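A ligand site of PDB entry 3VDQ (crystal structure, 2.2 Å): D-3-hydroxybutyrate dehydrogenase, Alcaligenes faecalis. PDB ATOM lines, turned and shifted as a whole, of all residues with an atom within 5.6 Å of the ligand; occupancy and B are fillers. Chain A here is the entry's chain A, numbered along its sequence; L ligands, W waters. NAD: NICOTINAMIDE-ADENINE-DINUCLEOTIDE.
The side-chain amide nitrogen of Asn 90 sits at hydrogen-bond distance from the backbone carbonyl oxygen of Gly 11. The side-chain amide nitrogen (ND2) of Asn 90 sits close to the backbone NH (N) of Gly 17 (3.4 Å). The side-chain hydroxyl (OG1) of Thr 10 sits at hydrogen-bond distance from the backbone NH (N) of Asn 90, 2.7 Å away. The side-chain carboxylate (OD2) of Asp 63 is in hydrogen-bond range of the side-chain hydroxyl (OG) of Ser 65 (2.6 Å). O of Ile 140 lies within hydrogen-bond range of NZ of Lys 159, 3.1 Å away. The backbone carbonyl oxygen (O) of Phe 36 is in hydrogen-bond range of the side-chain hydroxyl (OG1) of Thr 13, at 2.8 Å. N of Gly 11 is in hydrogen-bond range of OD1 of Asn 34, at 2.9 Å. O of Pro 185 is in hydrogen-bond range of N of Ala 143.
Water W5 bridges OG of Ser 14 (2.6 Å) and O2A of the ligand (2.7 Å). Water W3 bridges OG of Ser 142 (2.5 Å) and OH of Tyr 155 (2.6 Å). Water W2 bridges O of Gly 92 (2.8 Å) and O1A of the ligand (3.2 Å).
O3D of the ligand sits at hydrogen-bond distance from O of Asn 90 (2.6 Å). An oxygen (O7N) of the ligand is in hydrogen-bond range of the backbone NH of Val 188 (2.6 Å). N7N of the ligand lies within hydrogen-bond range of O of Val 188. The side-chain hydroxyl (OG1) of Thr 190 sits at hydrogen-bond distance from an oxygen (O1N) of the ligand (2.7 Å). A nitrogen (N6A) of the ligand lies within hydrogen-bond range of the side-chain carboxylate of Asp 63 (2.7 Å). The side-chain amino group (NZ) of Lys 159 sits at hydrogen-bond distance from an oxygen (O2D) of the ligand, at 2.8 Å. The side-chain hydroxyl of Tyr 155 sits at hydrogen-bond distance from an oxygen (O2D) of the ligand, at 2.9 Å. The backbone NH (N) of Ser 14 lies within hydrogen-bond range of an oxygen (O3B) of the ligand (3.3 Å). O3B of the ligand lies within hydrogen-bond range of OG of Ser 14 (3.0 Å). The side-chain hydroxyl (OG1) of Thr 13 is in hydrogen-bond range of an oxygen (O3B) of the ligand, at 3.0 Å. O2N of the ligand sits at hydrogen-bond distance from N of Ile 16, at 3.2 Å. The backbone NH (N) of Leu 64 sits at hydrogen-bond distance from a nitrogen (N1A) of the ligand (3.3 Å). The backbone NH (N) of Gly 92 lies close to an oxygen (O3D) of the ligand (3.5 Å).
CA of Gly 11 touches O4B of the ligand, 3.1 Å away. Gly 15 touches the ligand (CA to O2A, 3.7 Å). Asn 34 touches the ligand (OD1 to C2A, 3.8 Å). Phe 36 touches the ligand. Ala 62 touches the ligand (O to N1A, 3.9 Å). Ser 65 touches the ligand. Ala 91 touches the ligand (CB to N3A, 3.2 Å). CD1 of Leu 113 touches N1A of the ligand, 3.6 Å away. Ile 140 touches the ligand (CG2 to O4D, 3.6 Å). O of Ala 141 touches C6N of the ligand, 3.3 Å away. OG of Ser 142 touches C5N of the ligand, at 3.5 Å. O of Pro 185 touches C5N of the ligand (3.5 Å). Gly 186 touches the ligand (O to C4N, 3.2 Å). C of Trp 187 touches O7N of the ligand, 3.5 Å away. CD of Pro 191 touches O2A of the ligand (3.4 Å). Leu 192 touches the ligand (CB to O3, 3.6 Å). Val 193 touches the ligand (CG2 to O7N, 3.1 Å). Hydrophobic or aromatic side chains within 4 Å of the ligand: Ile 16, Phe 36, Leu 64, Ala 91, Leu 113, Ile 140, Tyr 155, Pro 185, Trp 187, Val 188, Pro 191, Leu 192 and Val 193. Within 4 Å of the ligand: Gly 11, Thr 13, Ser 14, Gly 15, Ile 16, Asn 34, Phe 36, Ala 62, Asp 63, Leu 64, Ser 65, Asn 90, Ala 91, Gly 92, Leu 113, Ile 140, Ala 141, Ser 142, Tyr 155, Lys 159, Pro 185, Gly 186, Trp 187, Val 188, Thr 190, Pro 191, Leu 192 and Val 193.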
ATOM      1  N   THR A  10      23.371  21.583 -21.871  1.00  0.00           N
ATOM      2  CA  THR A  10      22.769  22.339 -20.773  1.00  0.00           C
ATOM      3  C   THR A  10      21.741  21.476 -20.050  1.00  0.00           C
ATOM      4  O   THR A  10      21.144  20.585 -20.648  1.00  0.00           O
ATOM      5  CB  THR A  10      22.100  23.645 -21.278  1.00  0.00           C
ATOM      6  OG1 THR A  10      21.039  23.321 -22.191  1.00  0.00           O
ATOM      7  CG2 THR A  10      23.119  24.496 -22.003  1.00  0.00           C
ATOM      8  N   GLY A  11      21.532  21.737 -18.764  1.00  0.00           N
ATOM      9  CA  GLY A  11      20.586  20.947 -17.995  1.00  0.00           C
ATOM     10  C   GLY A  11      20.911  19.460 -18.106  1.00  0.00           C
ATOM     11  O   GLY A  11      20.014  18.639 -18.336  1.00  0.00           O
ATOM     12  N   SER A  12      22.182  19.110 -17.928  1.00  0.00           N
ATOM     13  CA  SER A  12      22.616  17.722 -18.059  1.00  0.00           C
ATOM     14  C   SER A  12      23.051  16.983 -16.794  1.00  0.00           C
ATOM     15  O   SER A  12      23.680  15.927 -16.885  1.00  0.00           O
ATOM     16  CB  SER A  12      23.745  17.622 -19.095  1.00  0.00           C
ATOM     17  OG  SER A  12      24.755  18.567 -18.840  1.00  0.00           O
ATOM     18  N   THR A  13      22.714  17.501 -15.623  1.00  0.00           N
ATOM     19  CA  THR A  13      23.086  16.810 -14.386  1.00  0.00           C
ATOM     20  C   THR A  13      22.065  15.712 -14.044  1.00  0.00           C
ATOM     21  O   THR A  13      22.305  14.885 -13.166  1.00  0.00           O
ATOM     22  CB  THR A  13      23.204  17.783 -13.200  1.00  0.00           C
ATOM     23  OG1 THR A  13      22.013  18.573 -13.083  1.00  0.00           O
ATOM     24  CG2 THR A  13      24.395  18.708 -13.407  1.00  0.00           C
ATOM     25  N   SER A  14      20.947  15.701 -14.764  1.00  0.00           N
ATOM     26  CA  SER A  14      19.909  14.692 -14.569  1.00  0.00           C
ATOM     27  C   SER A  14      18.941  14.658 -15.748  1.00  0.00           C
ATOM     28  O   SER A  14      19.026  15.494 -16.656  1.00  0.00           O
ATOM     29  CB  SER A  14      19.133  14.962 -13.274  1.00  0.00           C
ATOM     30  OG  SER A  14      18.507  16.230 -13.289  1.00  0.00           O
ATOM     31  N   GLY A  15      18.041  13.684 -15.745  1.00  0.00           N
ATOM     32  CA  GLY A  15      17.053  13.543 -16.813  1.00  0.00           C
ATOM     33  C   GLY A  15      17.596  13.310 -18.218  1.00  0.00           C
ATOM     34  O   GLY A  15      18.564  12.571 -18.422  1.00  0.00           O
ATOM     35  N   ILE A  16      16.951  13.952 -19.199  1.00  0.00           N
ATOM     36  CA  ILE A  16      17.333  13.839 -20.598  1.00  0.00           C
ATOM     37  C   ILE A  16      18.735  14.368 -20.889  1.00  0.00           C
ATOM     38  O   ILE A  16      19.498  13.763 -21.637  1.00  0.00           O
ATOM     39  CB  ILE A  16      16.313  14.573 -21.478  1.00  0.00           C
ATOM     40  CG1 ILE A  16      14.957  13.878 -21.379  1.00  0.00           C
ATOM     41  CG2 ILE A  16      16.800  14.615 -22.929  1.00  0.00           C
ATOM     42  CD1 ILE A  16      13.849  14.602 -22.079  1.00  0.00           C
ATOM     43  N   GLY A  17      19.066  15.517 -20.311  1.00  0.00           N
ATOM     44  CA  GLY A  17      20.372  16.109 -20.525  1.00  0.00           C
ATOM     45  C   GLY A  17      21.533  15.173 -20.191  1.00  0.00           C
ATOM     46  O   GLY A  17      22.514  15.099 -20.932  1.00  0.00           O
ATOM     47  N   ASN A  34      26.242  20.427 -17.278  1.00  0.00           N
ATOM     48  CA  ASN A  34      25.781  21.611 -16.550  1.00  0.00           C
ATOM     49  C   ASN A  34      24.427  21.402 -15.878  1.00  0.00           C
ATOM     50  O   ASN A  34      23.625  20.593 -16.329  1.00  0.00           O
ATOM     51  CB  ASN A  34      25.719  22.816 -17.510  1.00  0.00           C
ATOM     52  CG  ASN A  34      24.581  23.784 -17.200  1.00  0.00           C
ATOM     53  OD1 ASN A  34      23.434  23.552 -17.610  1.00  0.00           O
ATOM     54  ND2 ASN A  34      24.878  24.860 -16.490  1.00  0.00           N
ATOM     55  N   GLY A  35      24.190  22.141 -14.798  1.00  0.00           N
ATOM     56  CA  GLY A  35      22.933  22.021 -14.084  1.00  0.00           C
ATOM     57  C   GLY A  35      23.068  22.124 -12.573  1.00  0.00           C
ATOM     58  O   GLY A  35      24.119  22.486 -12.053  1.00  0.00           O
ATOM     59  N   PHE A  36      21.982  21.801 -11.869  1.00  0.00           N
ATOM     60  CA  PHE A  36      21.959  21.863 -10.427  1.00  0.00           C
ATOM     61  C   PHE A  36      21.899  20.479  -9.792  1.00  0.00           C
ATOM     62  O   PHE A  36      21.787  19.470 -10.485  1.00  0.00           O
ATOM     63  CB  PHE A  36      20.752  22.701  -9.972  1.00  0.00           C
ATOM     64  CG  PHE A  36      20.815  24.140 -10.431  1.00  0.00           C
ATOM     65  CD1 PHE A  36      20.142  24.542 -11.577  1.00  0.00           C
ATOM     66  CD2 PHE A  36      21.588  25.065  -9.739  1.00  0.00           C
ATOM     67  CE1 PHE A  36      20.236  25.862 -12.025  1.00  0.00           C
ATOM     68  CE2 PHE A  36      21.685  26.390 -10.180  1.00  0.00           C
ATOM     69  CZ  PHE A  36      21.008  26.786 -11.334  1.00  0.00           C
ATOM     70  N   GLY A  37      21.982  20.437  -8.457  1.00  0.00           N
ATOM     71  CA  GLY A  37      21.921  19.169  -7.742  1.00  0.00           C
ATOM     72  C   GLY A  37      23.030  19.014  -6.706  1.00  0.00           C
ATOM     73  O   GLY A  37      23.842  19.932  -6.526  1.00  0.00           O
ATOM     74  N   ALA A  62      25.867  27.009 -13.798  1.00  0.00           N
ATOM     75  CA  ALA A  62      25.429  28.311 -14.299  1.00  0.00           C
ATOM     76  C   ALA A  62      23.913  28.307 -14.431  1.00  0.00           C
ATOM     77  O   ALA A  62      23.315  27.321 -14.872  1.00  0.00           O
ATOM     78  CB  ALA A  62      26.079  28.606 -15.649  1.00  0.00           C
ATOM     79  N   ASP A  63      23.297  29.412 -14.026  1.00  0.00           N
ATOM     80  CA  ASP A  63      21.860  29.540 -14.123  1.00  0.00           C
ATOM     81  C   ASP A  63      21.592  30.153 -15.494  1.00  0.00           C
ATOM     82  O   ASP A  63      21.698  31.375 -15.676  1.00  0.00           O
ATOM     83  CB  ASP A  63      21.310  30.437 -13.021  1.00  0.00           C
ATOM     84  CG  ASP A  63      19.804  30.578 -13.084  1.00  0.00           C
ATOM     85  OD1 ASP A  63      19.213  31.173 -12.154  1.00  0.00           O
ATOM     86  OD2 ASP A  63      19.204  30.096 -14.069  1.00  0.00           O
ATOM     87  N   LEU A  64      21.256  29.303 -16.452  1.00  0.00           N
ATOM     88  CA  LEU A  64      20.997  29.741 -17.806  1.00  0.00           C
ATOM     89  C   LEU A  64      19.767  30.631 -17.946  1.00  0.00           C
ATOM     90  O   LEU A  64      19.490  31.140 -19.025  1.00  0.00           O
ATOM     91  CB  LEU A  64      20.900  28.524 -18.727  1.00  0.00           C
ATOM     92  CG  LEU A  64      22.162  27.657 -18.603  1.00  0.00           C
ATOM     93  CD1 LEU A  64      22.083  26.461 -19.519  1.00  0.00           C
ATOM     94  CD2 LEU A  64      23.390  28.502 -18.939  1.00  0.00           C
ATOM     95  N   SER A  65      19.031  30.833 -16.851  1.00  0.00           N
ATOM     96  CA  SER A  65      17.860  31.693 -16.897  1.00  0.00           C
ATOM     97  C   SER A  65      18.368  33.141 -16.988  1.00  0.00           C
ATOM     98  O   SER A  65      17.595  34.074 -17.171  1.00  0.00           O
ATOM     99  CB  SER A  65      16.990  31.531 -15.648  1.00  0.00           C
ATOM    100  OG  SER A  65      17.602  32.121 -14.510  1.00  0.00           O
ATOM    101  N   ASN A  90      19.401  22.023 -23.834  1.00  0.00           N
ATOM    102  CA  ASN A  90      18.435  21.114 -23.220  1.00  0.00           C
ATOM    103  C   ASN A  90      17.717  21.621 -21.971  1.00  0.00           C
ATOM    104  O   ASN A  90      16.540  21.354 -21.786  1.00  0.00           O
ATOM    105  CB  ASN A  90      19.137  19.781 -22.912  1.00  0.00           C
ATOM    106  CG  ASN A  90      18.285  18.845 -22.068  1.00  0.00           C
ATOM    107  OD1 ASN A  90      17.437  18.114 -22.585  1.00  0.00           O
ATOM    108  ND2 ASN A  90      18.511  18.878 -20.764  1.00  0.00           N
ATOM    109  N   ALA A  91      18.429  22.350 -21.109  1.00  0.00           N
ATOM    110  CA  ALA A  91      17.835  22.832 -19.872  1.00  0.00           C
ATOM    111  C   ALA A  91      16.464  23.488 -20.021  1.00  0.00           C
ATOM    112  O   ALA A  91      16.290  24.402 -20.819  1.00  0.00           O
ATOM    113  CB  ALA A  91      18.786  23.784 -19.174  1.00  0.00           C
ATOM    114  N   GLY A  92      15.500  23.022 -19.231  1.00  0.00           N
ATOM    115  CA  GLY A  92      14.162  23.587 -19.288  1.00  0.00           C
ATOM    116  C   GLY A  92      13.348  23.288 -18.041  1.00  0.00           C
ATOM    117  O   GLY A  92      13.692  22.404 -17.259  1.00  0.00           O
ATOM    118  N   ILE A  93      12.271  24.035 -17.845  1.00  0.00           N
ATOM    119  CA  ILE A  93      11.406  23.823 -16.692  1.00  0.00           C
ATOM    120  C   ILE A  93       9.948  23.857 -17.122  1.00  0.00           C
ATOM    121  O   ILE A  93       9.632  24.285 -18.234  1.00  0.00           O
ATOM    122  CB  ILE A  93      11.649  24.875 -15.583  1.00  0.00           C
ATOM    123  CG1 ILE A  93      11.554  26.283 -16.167  1.00  0.00           C
ATOM    124  CG2 ILE A  93      13.022  24.650 -14.951  1.00  0.00           C
ATOM    125  CD1 ILE A  93      11.622  27.370 -15.117  1.00  0.00           C
ATOM    126  N   LEU A 113      14.405  30.595 -19.405  1.00  0.00           N
ATOM    127  CA  LEU A 113      15.232  29.395 -19.542  1.00  0.00           C
ATOM    128  C   LEU A 113      14.924  28.609 -20.800  1.00  0.00           C
ATOM    129  O   LEU A 113      15.802  28.310 -21.609  1.00  0.00           O
ATOM    130  CB  LEU A 113      15.032  28.483 -18.327  1.00  0.00           C
ATOM    131  CG  LEU A 113      15.883  27.221 -18.436  1.00  0.00           C
ATOM    132  CD1 LEU A 113      17.358  27.630 -18.459  1.00  0.00           C
ATOM    133  CD2 LEU A 113      15.587  26.284 -17.266  1.00  0.00           C
ATOM    134  N   ASN A 114      13.652  28.267 -20.978  1.00  0.00           N
ATOM    135  CA  ASN A 114      13.208  27.486 -22.119  1.00  0.00           C
ATOM    136  C   ASN A 114      13.366  28.112 -23.491  1.00  0.00           C
ATOM    137  O   ASN A 114      13.463  27.387 -24.482  1.00  0.00           O
ATOM    138  CB  ASN A 114      11.755  27.078 -21.907  1.00  0.00           C
ATOM    139  CG  ASN A 114      11.598  26.100 -20.769  1.00  0.00           C
ATOM    140  OD1 ASN A 114      12.264  26.226 -19.743  1.00  0.00           O
ATOM    141  ND2 ASN A 114      10.710  25.123 -20.944  1.00  0.00           N
ATOM    142  N   ILE A 140      16.545  21.249 -27.864  1.00  0.00           N
ATOM    143  CA  ILE A 140      15.565  20.311 -27.376  1.00  0.00           C
ATOM    144  C   ILE A 140      14.261  21.027 -27.116  1.00  0.00           C
ATOM    145  O   ILE A 140      14.067  21.686 -26.093  1.00  0.00           O
ATOM    146  CB  ILE A 140      16.072  19.609 -26.126  1.00  0.00           C
ATOM    147  CG1 ILE A 140      17.287  18.758 -26.502  1.00  0.00           C
ATOM    148  CG2 ILE A 140      14.956  18.756 -25.509  1.00  0.00           C
ATOM    149  CD1 ILE A 140      17.822  17.904 -25.396  1.00  0.00           C
ATOM    150  N   ALA A 141      13.358  20.889 -28.085  1.00  0.00           N
ATOM    151  CA  ALA A 141      12.061  21.502 -27.989  1.00  0.00           C
ATOM    152  C   ALA A 141      11.107  20.515 -27.358  1.00  0.00           C
ATOM    153  O   ALA A 141      11.338  20.064 -26.245  1.00  0.00           O
ATOM    154  CB  ALA A 141      11.580  21.905 -29.379  1.00  0.00           C
ATOM    155  N   SER A 142      10.050  20.170 -28.085  1.00  0.00           N
ATOM    156  CA  SER A 142       9.049  19.254 -27.577  1.00  0.00           C
ATOM    157  C   SER A 142       7.930  19.117 -28.592  1.00  0.00           C
ATOM    158  O   SER A 142       7.823  19.910 -29.518  1.00  0.00           O
ATOM    159  CB  SER A 142       8.478  19.834 -26.272  1.00  0.00           C
ATOM    160  OG  SER A 142       7.321  19.145 -25.850  1.00  0.00           O
ATOM    161  N   ALA A 143       7.097  18.102 -28.418  1.00  0.00           N
ATOM    162  CA  ALA A 143       5.958  17.939 -29.309  1.00  0.00           C
ATOM    163  C   ALA A 143       5.142  19.207 -29.094  1.00  0.00           C
ATOM    164  O   ALA A 143       4.388  19.649 -29.969  1.00  0.00           O
ATOM    165  CB  ALA A 143       5.133  16.706 -28.905  1.00  0.00           C
ATOM    166  N   TYR A 155       5.056  27.308 -21.647  1.00  0.00           N
ATOM    167  CA  TYR A 155       5.883  26.240 -22.175  1.00  0.00           C
ATOM    168  C   TYR A 155       5.648  25.990 -23.655  1.00  0.00           C
ATOM    169  O   TYR A 155       6.610  25.873 -24.423  1.00  0.00           O
ATOM    170  CB  TYR A 155       5.631  24.974 -21.345  1.00  0.00           C
ATOM    171  CG  TYR A 155       6.502  23.776 -21.676  1.00  0.00           C
ATOM    172  CD1 TYR A 155       6.159  22.910 -22.708  1.00  0.00           C
ATOM    173  CD2 TYR A 155       7.641  23.486 -20.918  1.00  0.00           C
ATOM    174  CE1 TYR A 155       6.919  21.772 -22.979  1.00  0.00           C
ATOM    175  CE2 TYR A 155       8.396  22.360 -21.182  1.00  0.00           C
ATOM    176  CZ  TYR A 155       8.033  21.500 -22.210  1.00  0.00           C
ATOM    177  OH  TYR A 155       8.770  20.369 -22.462  1.00  0.00           O
ATOM    178  N   LYS A 159       8.413  26.582 -26.375  1.00  0.00           N
ATOM    179  CA  LYS A 159       8.789  25.455 -27.226  1.00  0.00           C
ATOM    180  C   LYS A 159       8.537  25.797 -28.686  1.00  0.00           C
ATOM    181  O   LYS A 159       9.335  25.427 -29.555  1.00  0.00           O
ATOM    182  CB  LYS A 159       8.025  24.185 -26.838  1.00  0.00           C
ATOM    183  CG  LYS A 159       8.484  23.575 -25.524  1.00  0.00           C
ATOM    184  CD  LYS A 159       9.998  23.374 -25.514  1.00  0.00           C
ATOM    185  CE  LYS A 159      10.484  22.909 -24.164  1.00  0.00           C
ATOM    186  NZ  LYS A 159      11.960  22.825 -24.123  1.00  0.00           N
ATOM    187  N   PRO A 185      10.657  15.724 -28.385  1.00  0.00           N
ATOM    188  CA  PRO A 185      10.235  14.525 -27.661  1.00  0.00           C
ATOM    189  C   PRO A 185       8.792  14.514 -27.210  1.00  0.00           C
ATOM    190  O   PRO A 185       8.171  15.561 -27.003  1.00  0.00           O
ATOM    191  CB  PRO A 185      11.186  14.495 -26.461  1.00  0.00           C
ATOM    192  CG  PRO A 185      12.333  15.393 -26.869  1.00  0.00           C
ATOM    193  CD  PRO A 185      11.635  16.482 -27.603  1.00  0.00           C
ATOM    194  N   GLY A 186       8.259  13.307 -27.069  1.00  0.00           N
ATOM    195  CA  GLY A 186       6.922  13.133 -26.550  1.00  0.00           C
ATOM    196  C   GLY A 186       7.188  12.905 -25.065  1.00  0.00           C
ATOM    197  O   GLY A 186       8.200  13.379 -24.535  1.00  0.00           O
ATOM    198  N   TRP A 187       6.316  12.163 -24.382  1.00  0.00           N
ATOM    199  CA  TRP A 187       6.479  11.883 -22.959  1.00  0.00           C
ATOM    200  C   TRP A 187       7.749  11.112 -22.597  1.00  0.00           C
ATOM    201  O   TRP A 187       7.983  10.023 -23.101  1.00  0.00           O
ATOM    202  CB  TRP A 187       5.291  11.088 -22.434  1.00  0.00           C
ATOM    203  CG  TRP A 187       4.014  11.851 -22.339  1.00  0.00           C
ATOM    204  CD1 TRP A 187       2.795  11.475 -22.842  1.00  0.00           C
ATOM    205  CD2 TRP A 187       3.787  13.080 -21.637  1.00  0.00           C
ATOM    206  NE1 TRP A 187       1.832  12.393 -22.488  1.00  0.00           N
ATOM    207  CE2 TRP A 187       2.420  13.383 -21.747  1.00  0.00           C
ATOM    208  CE3 TRP A 187       4.622  13.957 -20.918  1.00  0.00           C
ATOM    209  CZ2 TRP A 187       1.853  14.534 -21.166  1.00  0.00           C
ATOM    210  CZ3 TRP A 187       4.054  15.090 -20.339  1.00  0.00           C
ATOM    211  CH2 TRP A 187       2.692  15.367 -20.472  1.00  0.00           C
ATOM    212  N   VAL A 188       8.544  11.692 -21.705  1.00  0.00           N
ATOM    213  CA  VAL A 188       9.766  11.052 -21.204  1.00  0.00           C
ATOM    214  C   VAL A 188       9.568  11.084 -19.683  1.00  0.00           C
ATOM    215  O   VAL A 188       9.408  12.161 -19.105  1.00  0.00           O
ATOM    216  CB  VAL A 188      11.046  11.849 -21.558  1.00  0.00           C
ATOM    217  CG1 VAL A 188      12.282  11.042 -21.160  1.00  0.00           C
ATOM    218  CG2 VAL A 188      11.078  12.169 -23.049  1.00  0.00           C
ATOM    219  N   ARG A 189       9.570   9.916 -19.045  1.00  0.00           N
ATOM    220  CA  ARG A 189       9.332   9.859 -17.615  1.00  0.00           C
ATOM    221  C   ARG A 189      10.494  10.300 -16.729  1.00  0.00           C
ATOM    222  O   ARG A 189      11.201   9.489 -16.131  1.00  0.00           O
ATOM    223  CB  ARG A 189       8.854   8.464 -17.208  1.00  0.00           C
ATOM    224  CG  ARG A 189       8.255   8.440 -15.808  1.00  0.00           C
ATOM    225  CD  ARG A 189       7.527   7.141 -15.517  1.00  0.00           C
ATOM    226  NE  ARG A 189       6.805   7.222 -14.242  1.00  0.00           N
ATOM    227  CZ  ARG A 189       5.975   6.287 -13.782  1.00  0.00           C
ATOM    228  NH1 ARG A 189       5.764   5.175 -14.482  1.00  0.00           N
ATOM    229  NH2 ARG A 189       5.364   6.475 -12.619  1.00  0.00           N
ATOM    230  N   THR A 190      10.655  11.614 -16.666  1.00  0.00           N
ATOM    231  CA  THR A 190      11.700  12.250 -15.876  1.00  0.00           C
ATOM    232  C   THR A 190      10.977  12.945 -14.714  1.00  0.00           C
ATOM    233  O   THR A 190       9.745  12.912 -14.649  1.00  0.00           O
ATOM    234  CB  THR A 190      12.425  13.316 -16.708  1.00  0.00           C
ATOM    235  OG1 THR A 190      11.485  14.303 -17.141  1.00  0.00           O
ATOM    236  CG2 THR A 190      13.095  12.676 -17.931  1.00  0.00           C
ATOM    237  N   PRO A 191      11.725  13.567 -13.790  1.00  0.00           N
ATOM    238  CA  PRO A 191      11.052  14.239 -12.673  1.00  0.00           C
ATOM    239  C   PRO A 191      10.028  15.281 -13.129  1.00  0.00           C
ATOM    240  O   PRO A 191       8.939  15.394 -12.566  1.00  0.00           O
ATOM    241  CB  PRO A 191      12.219  14.863 -11.902  1.00  0.00           C
ATOM    242  CG  PRO A 191      13.314  13.838 -12.108  1.00  0.00           C
ATOM    243  CD  PRO A 191      13.184  13.540 -13.590  1.00  0.00           C
ATOM    244  N   LEU A 192      10.386  16.040 -14.167  1.00  0.00           N
ATOM    245  CA  LEU A 192       9.504  17.068 -14.725  1.00  0.00           C
ATOM    246  C   LEU A 192       8.117  16.492 -15.059  1.00  0.00           C
ATOM    247  O   LEU A 192       7.110  17.190 -14.950  1.00  0.00           O
ATOM    248  CB  LEU A 192      10.158  17.675 -15.981  1.00  0.00           C
ATOM    249  CG  LEU A 192       9.484  18.862 -16.661  1.00  0.00           C
ATOM    250  CD1 LEU A 192      10.477  19.519 -17.604  1.00  0.00           C
ATOM    251  CD2 LEU A 192       8.237  18.411 -17.417  1.00  0.00           C
ATOM    252  N   VAL A 193       8.079  15.228 -15.466  1.00  0.00           N
ATOM    253  CA  VAL A 193       6.830  14.551 -15.809  1.00  0.00           C
ATOM    254  C   VAL A 193       6.229  13.779 -14.636  1.00  0.00           C
ATOM    255  O   VAL A 193       5.003  13.699 -14.494  1.00  0.00           O
ATOM    256  CB  VAL A 193       7.039  13.579 -16.996  1.00  0.00           C
ATOM    257  CG1 VAL A 193       5.852  12.637 -17.141  1.00  0.00           C
ATOM    258  CG2 VAL A 193       7.237  14.373 -18.263  1.00  0.00           C
HETATM  259  PA  NAD L   1      14.558  17.493 -15.726  1.00  0.00           P
HETATM  260  O1A NAD L   1      13.906  18.142 -14.629  1.00  0.00           O
HETATM  261  O2A NAD L   1      14.561  16.009 -15.555  1.00  0.00           O
HETATM  262  O5B NAD L   1      15.935  18.132 -16.148  1.00  0.00           O
HETATM  263  C5B NAD L   1      16.201  19.580 -16.175  1.00  0.00           C
HETATM  264  C4B NAD L   1      17.779  19.650 -16.121  1.00  0.00           C
HETATM  265  O4B NAD L   1      18.067  21.124 -16.135  1.00  0.00           O
HETATM  266  C3B NAD L   1      18.122  19.221 -14.733  1.00  0.00           C
HETATM  267  O3B NAD L   1      19.458  18.699 -14.701  1.00  0.00           O
HETATM  268  C2B NAD L   1      17.983  20.514 -13.971  1.00  0.00           C
HETATM  269  O2B NAD L   1      18.503  20.546 -12.615  1.00  0.00           O
HETATM  270  C1B NAD L   1      18.644  21.580 -14.826  1.00  0.00           C
HETATM  271  N9A NAD L   1      18.141  22.916 -14.710  1.00  0.00           N
HETATM  272  C8A NAD L   1      17.316  23.487 -13.716  1.00  0.00           C
HETATM  273  N7A NAD L   1      17.247  24.809 -13.773  1.00  0.00           N
HETATM  274  C5A NAD L   1      18.184  25.181 -14.681  1.00  0.00           C
HETATM  275  C6A NAD L   1      18.683  26.440 -15.138  1.00  0.00           C
HETATM  276  N6A NAD L   1      18.170  27.644 -14.675  1.00  0.00           N
HETATM  277  N1A NAD L   1      19.725  26.422 -16.038  1.00  0.00           N
HETATM  278  C2A NAD L   1      20.271  25.274 -16.500  1.00  0.00           C
HETATM  279  N3A NAD L   1      19.832  24.018 -16.119  1.00  0.00           N
HETATM  280  C4A NAD L   1      18.785  24.043 -15.234  1.00  0.00           C
HETATM  281  O3  NAD L   1      13.578  17.846 -16.950  1.00  0.00           O
HETATM  282  PN  NAD L   1      13.737  17.105 -18.357  1.00  0.00           P
HETATM  283  O1N NAD L   1      12.530  16.307 -18.545  1.00  0.00           O
HETATM  284  O2N NAD L   1      14.923  16.255 -18.386  1.00  0.00           O
HETATM  285  O5D NAD L   1      13.832  18.210 -19.509  1.00  0.00           O
HETATM  286  C5D NAD L   1      15.049  18.292 -20.282  1.00  0.00           C
HETATM  287  C4D NAD L   1      14.620  18.886 -21.636  1.00  0.00           C
HETATM  288  O4D NAD L   1      13.654  17.913 -22.216  1.00  0.00           O
HETATM  289  C3D NAD L   1      13.852  20.197 -21.418  1.00  0.00           C
HETATM  290  O3D NAD L   1      13.993  21.546 -21.979  1.00  0.00           O
HETATM  291  C2D NAD L   1      12.360  19.777 -21.455  1.00  0.00           C
HETATM  292  O2D NAD L   1      11.694  20.629 -22.431  1.00  0.00           O
HETATM  293  C1D NAD L   1      12.484  18.691 -22.462  1.00  0.00           C
HETATM  294  N1N NAD L   1      11.329  17.781 -22.665  1.00  0.00           N
HETATM  295  C2N NAD L   1      10.972  16.845 -21.669  1.00  0.00           C
HETATM  296  C3N NAD L   1       9.892  15.994 -21.877  1.00  0.00           C
HETATM  297  C7N NAD L   1       9.456  14.994 -20.883  1.00  0.00           C
HETATM  298  O7N NAD L   1       8.443  14.265 -21.144  1.00  0.00           O
HETATM  299  N7N NAD L   1      10.123  14.870 -19.718  1.00  0.00           N
HETATM  300  C4N NAD L   1       9.139  16.071 -23.102  1.00  0.00           C
HETATM  301  C5N NAD L   1       9.526  17.042 -24.120  1.00  0.00           C
HETATM  302  C6N NAD L   1      10.648  17.912 -23.904  1.00  0.00           C
HETATM  303  O   HOH W   1      15.609  28.563 -13.612  1.00  0.00           O
HETATM  304  O   HOH W   2      12.811  21.094 -14.891  1.00  0.00           O
HETATM  305  O   HOH W   3       7.030  18.633 -23.372  1.00  0.00           O
HETATM  306  O   HOH W   4      17.576  17.002 -18.675  1.00  0.00           O
HETATM  307  O   HOH W   5      16.033  15.503 -13.373  1.00  0.00           O
